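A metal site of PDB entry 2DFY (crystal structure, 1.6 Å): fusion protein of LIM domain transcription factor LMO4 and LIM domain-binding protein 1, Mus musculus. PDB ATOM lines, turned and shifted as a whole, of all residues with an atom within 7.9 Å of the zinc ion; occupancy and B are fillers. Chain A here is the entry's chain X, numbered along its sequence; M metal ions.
Of the 16 residues printed, 4 come within 4 Å of the zinc ion. The nearest printed residue that does not touch the zinc ion is Thr 100 (4.7 Å).
The zinc ion is bound by OD2 of Asp 123, SG of Cys 120, SG of Cys 98 and SG of Cys 101.
SG of Cys 120 sits close to N of His 122 (3.6 Å). SG of Cys 98 sits close to N of Thr 100. The backbone NH (N) of Cys 98 is in hydrogen-bond range of the backbone carbonyl oxygen (O) of Asn 103 (2.8 Å). The side-chain sulfur (SG) of Cys 101 lies close to the backbone NH (N) of Asn 103.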
ATOM      1  N   THR A  97     -13.157 -21.550 -30.863  1.00  0.00           N
ATOM      2  CA  THR A  97     -12.073 -20.593 -30.534  1.00  0.00           C
ATOM      3  C   THR A  97     -11.536 -20.682 -29.088  1.00  0.00           C
ATOM      4  O   THR A  97     -12.192 -21.262 -28.192  1.00  0.00           O
ATOM      5  CB  THR A  97     -12.562 -19.159 -30.767  1.00  0.00           C
ATOM      6  OG1 THR A  97     -13.726 -18.896 -29.961  1.00  0.00           O
ATOM      7  CG2 THR A  97     -12.932 -18.952 -32.229  1.00  0.00           C
ATOM      8  N   CYS A  98     -10.339 -20.137 -28.853  1.00  0.00           N
ATOM      9  CA  CYS A  98      -9.783 -20.007 -27.491  1.00  0.00           C
ATOM     10  C   CYS A  98     -10.533 -18.937 -26.711  1.00  0.00           C
ATOM     11  O   CYS A  98     -10.688 -17.824 -27.171  1.00  0.00           O
ATOM     12  CB  CYS A  98      -8.282 -19.666 -27.500  1.00  0.00           C
ATOM     13  SG  CYS A  98      -7.583 -19.457 -25.819  1.00  0.00           S
ATOM     14  N   SER A  99     -11.032 -19.294 -25.530  1.00  0.00           N
ATOM     15  CA  SER A  99     -11.826 -18.366 -24.707  1.00  0.00           C
ATOM     16  C   SER A  99     -11.025 -17.157 -24.221  1.00  0.00           C
ATOM     17  O   SER A  99     -11.582 -16.088 -23.945  1.00  0.00           O
ATOM     18  CB  SER A  99     -12.402 -19.104 -23.511  1.00  0.00           C
ATOM     19  OG  SER A  99     -13.267 -20.161 -23.913  1.00  0.00           O
ATOM     20  N   THR A 100      -9.701 -17.322 -24.128  1.00  0.00           N
ATOM     21  CA  THR A 100      -8.820 -16.273 -23.655  1.00  0.00           C
ATOM     22  C   THR A 100      -8.312 -15.365 -24.799  1.00  0.00           C
ATOM     23  O   THR A 100      -8.576 -14.153 -24.795  1.00  0.00           O
ATOM     24  CB  THR A 100      -7.605 -16.894 -22.927  1.00  0.00           C
ATOM     25  OG1 THR A 100      -8.089 -17.635 -21.796  1.00  0.00           O
ATOM     26  CG2 THR A 100      -6.613 -15.826 -22.476  1.00  0.00           C
ATOM     27  N   CYS A 101      -7.607 -15.949 -25.763  1.00  0.00           N
ATOM     28  CA  CYS A 101      -7.000 -15.161 -26.846  1.00  0.00           C
ATOM     29  C   CYS A 101      -7.865 -15.019 -28.107  1.00  0.00           C
ATOM     30  O   CYS A 101      -7.582 -14.181 -28.968  1.00  0.00           O
ATOM     31  CB  CYS A 101      -5.614 -15.737 -27.215  1.00  0.00           C
ATOM     32  SG  CYS A 101      -5.615 -17.244 -28.245  1.00  0.00           S
ATOM     33  N   ARG A 102      -8.902 -15.846 -28.228  1.00  0.00           N
ATOM     34  CA  ARG A 102      -9.844 -15.807 -29.375  1.00  0.00           C
ATOM     35  C   ARG A 102      -9.327 -16.444 -30.677  1.00  0.00           C
ATOM     36  O   ARG A 102     -10.026 -16.394 -31.689  1.00  0.00           O
ATOM     37  CB  ARG A 102     -10.337 -14.390 -29.677  1.00  0.00           C
ATOM     38  CG  ARG A 102     -10.907 -13.670 -28.478  1.00  0.00           C
ATOM     39  CD  ARG A 102     -11.981 -12.675 -28.896  1.00  0.00           C
ATOM     40  NE  ARG A 102     -13.056 -13.318 -29.646  1.00  0.00           N
ATOM     41  CZ  ARG A 102     -13.991 -14.108 -29.124  1.00  0.00           C
ATOM     42  NH1 ARG A 102     -14.002 -14.378 -27.821  1.00  0.00           N
ATOM     43  NH2 ARG A 102     -14.921 -14.631 -29.913  1.00  0.00           N
ATOM     44  N   ASN A 103      -8.138 -17.035 -30.664  1.00  0.00           N
ATOM     45  CA  ASN A 103      -7.670 -17.791 -31.827  1.00  0.00           C
ATOM     46  C   ASN A 103      -8.624 -18.910 -32.190  1.00  0.00           C
ATOM     47  O   ASN A 103      -9.152 -19.587 -31.304  1.00  0.00           O
ATOM     48  CB  ASN A 103      -6.299 -18.412 -31.577  1.00  0.00           C
ATOM     49  CG  ASN A 103      -5.175 -17.474 -31.921  1.00  0.00           C
ATOM     50  OD1 ASN A 103      -5.362 -16.253 -31.950  1.00  0.00           O
ATOM     51  ND2 ASN A 103      -3.995 -18.026 -32.180  1.00  0.00           N
ATOM     52  N   ARG A 104      -8.818 -19.106 -33.494  1.00  0.00           N
ATOM     53  CA  ARG A 104      -9.568 -20.239 -34.010  1.00  0.00           C
ATOM     54  C   ARG A 104      -8.680 -21.480 -33.964  1.00  0.00           C
ATOM     55  O   ARG A 104      -7.563 -21.492 -34.482  1.00  0.00           O
ATOM     56  CB  ARG A 104     -10.013 -19.947 -35.442  1.00  0.00           C
ATOM     57  CG  ARG A 104     -10.929 -20.988 -36.050  1.00  0.00           C
ATOM     58  CD  ARG A 104     -11.217 -20.639 -37.502  1.00  0.00           C
ATOM     59  NE  ARG A 104     -11.526 -19.207 -37.667  1.00  0.00           N
ATOM     60  CZ  ARG A 104     -11.441 -18.532 -38.811  1.00  0.00           C
ATOM     61  NH1 ARG A 104     -11.069 -19.156 -39.937  1.00  0.00           N
ATOM     62  NH2 ARG A 104     -11.734 -17.235 -38.837  1.00  0.00           N
ATOM     63  N   LEU A 105      -9.226 -22.540 -33.352  1.00  0.00           N
ATOM     64  CA  LEU A 105      -8.500 -23.800 -33.208  1.00  0.00           C
ATOM     65  C   LEU A 105      -8.726 -24.656 -34.444  1.00  0.00           C
ATOM     66  O   LEU A 105      -9.836 -24.689 -34.981  1.00  0.00           O
ATOM     67  CB  LEU A 105      -9.012 -24.559 -31.983  1.00  0.00           C
ATOM     68  CG  LEU A 105      -9.121 -23.732 -30.716  1.00  0.00           C
ATOM     69  CD1 LEU A 105      -9.818 -24.566 -29.666  1.00  0.00           C
ATOM     70  CD2 LEU A 105      -7.758 -23.281 -30.257  1.00  0.00           C
ATOM     71  N   LEU A 118     -13.141 -23.262 -24.067  1.00  0.00           N
ATOM     72  CA  LEU A 118     -12.009 -23.801 -24.807  1.00  0.00           C
ATOM     73  C   LEU A 118     -10.800 -22.880 -24.641  1.00  0.00           C
ATOM     74  O   LEU A 118     -10.964 -21.656 -24.675  1.00  0.00           O
ATOM     75  CB  LEU A 118     -12.346 -23.889 -26.303  1.00  0.00           C
ATOM     76  CG  LEU A 118     -13.481 -24.826 -26.737  1.00  0.00           C
ATOM     77  CD1 LEU A 118     -14.029 -24.395 -28.104  1.00  0.00           C
ATOM     78  CD2 LEU A 118     -12.987 -26.241 -26.801  1.00  0.00           C
ATOM     79  N   PHE A 119      -9.619 -23.449 -24.462  1.00  0.00           N
ATOM     80  CA  PHE A 119      -8.387 -22.671 -24.342  1.00  0.00           C
ATOM     81  C   PHE A 119      -7.276 -23.310 -25.193  1.00  0.00           C
ATOM     82  O   PHE A 119      -7.116 -24.532 -25.196  1.00  0.00           O
ATOM     83  CB  PHE A 119      -7.928 -22.593 -22.889  1.00  0.00           C
ATOM     84  CG  PHE A 119      -9.006 -22.116 -21.937  1.00  0.00           C
ATOM     85  CD1 PHE A 119      -9.150 -20.781 -21.668  1.00  0.00           C
ATOM     86  CD2 PHE A 119      -9.870 -23.029 -21.333  1.00  0.00           C
ATOM     87  CE1 PHE A 119     -10.132 -20.323 -20.804  1.00  0.00           C
ATOM     88  CE2 PHE A 119     -10.864 -22.583 -20.454  1.00  0.00           C
ATOM     89  CZ  PHE A 119     -10.999 -21.228 -20.188  1.00  0.00           C
ATOM     90  N   CYS A 120      -6.507 -22.485 -25.899  1.00  0.00           N
ATOM     91  CA  CYS A 120      -5.438 -22.999 -26.722  1.00  0.00           C
ATOM     92  C   CYS A 120      -4.270 -23.399 -25.851  1.00  0.00           C
ATOM     93  O   CYS A 120      -4.238 -23.094 -24.650  1.00  0.00           O
ATOM     94  CB  CYS A 120      -4.997 -21.951 -27.725  1.00  0.00           C
ATOM     95  SG  CYS A 120      -4.045 -20.642 -26.960  1.00  0.00           S
ATOM     96  N   GLU A 121      -3.312 -24.101 -26.459  1.00  0.00           N
ATOM     97  CA  GLU A 121      -2.163 -24.669 -25.749  1.00  0.00           C
ATOM     98  C   GLU A 121      -1.394 -23.630 -24.930  1.00  0.00           C
ATOM     99  O   GLU A 121      -0.831 -23.944 -23.873  1.00  0.00           O
ATOM    100  CB  GLU A 121      -1.234 -25.317 -26.766  1.00  0.00           C
ATOM    101  CG  GLU A 121      -0.191 -26.238 -26.162  1.00  0.00           C
ATOM    102  CD  GLU A 121       0.890 -26.593 -27.169  1.00  0.00           C
ATOM    103  OE1 GLU A 121       0.565 -26.778 -28.371  1.00  0.00           O
ATOM    104  OE2 GLU A 121       2.061 -26.685 -26.750  1.00  0.00           O
ATOM    105  N   HIS A 122      -1.374 -22.388 -25.403  1.00  0.00           N
ATOM    106  CA  HIS A 122      -0.586 -21.328 -24.776  1.00  0.00           C
ATOM    107  C   HIS A 122      -1.427 -20.495 -23.813  1.00  0.00           C
ATOM    108  O   HIS A 122      -0.910 -19.557 -23.200  1.00  0.00           O
ATOM    109  CB  HIS A 122       0.076 -20.482 -25.860  1.00  0.00           C
ATOM    110  CG  HIS A 122       0.731 -21.304 -26.918  1.00  0.00           C
ATOM    111  ND1 HIS A 122       1.889 -22.021 -26.696  1.00  0.00           N
ATOM    112  CD2 HIS A 122       0.343 -21.597 -28.183  1.00  0.00           C
ATOM    113  CE1 HIS A 122       2.216 -22.681 -27.799  1.00  0.00           C
ATOM    114  NE2 HIS A 122       1.281 -22.449 -28.711  1.00  0.00           N
ATOM    115  N   ASP A 123      -2.695 -20.845 -23.666  1.00  0.00           N
ATOM    116  CA  ASP A 123      -3.568 -20.228 -22.676  1.00  0.00           C
ATOM    117  C   ASP A 123      -4.108 -21.247 -21.707  1.00  0.00           C
ATOM    118  O   ASP A 123      -5.257 -21.143 -21.285  1.00  0.00           O
ATOM    119  CB  ASP A 123      -4.714 -19.482 -23.351  1.00  0.00           C
ATOM    120  CG  ASP A 123      -4.281 -18.158 -23.933  1.00  0.00           C
ATOM    121  OD1 ASP A 123      -3.548 -17.409 -23.247  1.00  0.00           O
ATOM    122  OD2 ASP A 123      -4.683 -17.862 -25.070  1.00  0.00           O
ATOM    123  N   ARG A 124      -3.296 -22.240 -21.351  1.00  0.00           N
ATOM    124  CA  ARG A 124      -3.706 -23.201 -20.331  1.00  0.00           C
ATOM    125  C   ARG A 124      -4.204 -22.413 -19.110  1.00  0.00           C
ATOM    126  O   ARG A 124      -3.459 -21.596 -18.580  1.00  0.00           O
ATOM    127  CB  ARG A 124      -2.533 -24.114 -19.954  1.00  0.00           C
ATOM    128  CG  ARG A 124      -2.826 -25.139 -18.873  1.00  0.00           C
ATOM    129  CD  ARG A 124      -1.626 -26.020 -18.608  1.00  0.00           C
ATOM    130  NE  ARG A 124      -1.911 -27.049 -17.609  1.00  0.00           N
ATOM    131  CZ  ARG A 124      -1.884 -26.875 -16.293  1.00  0.00           C
ATOM    132  NH1 ARG A 124      -1.580 -25.700 -15.752  1.00  0.00           N
ATOM    133  NH2 ARG A 124      -2.171 -27.895 -15.493  1.00  0.00           N
HETATM  134 ZN    ZN M   1      -5.479 -18.879 -26.599  1.00  0.00          ZN
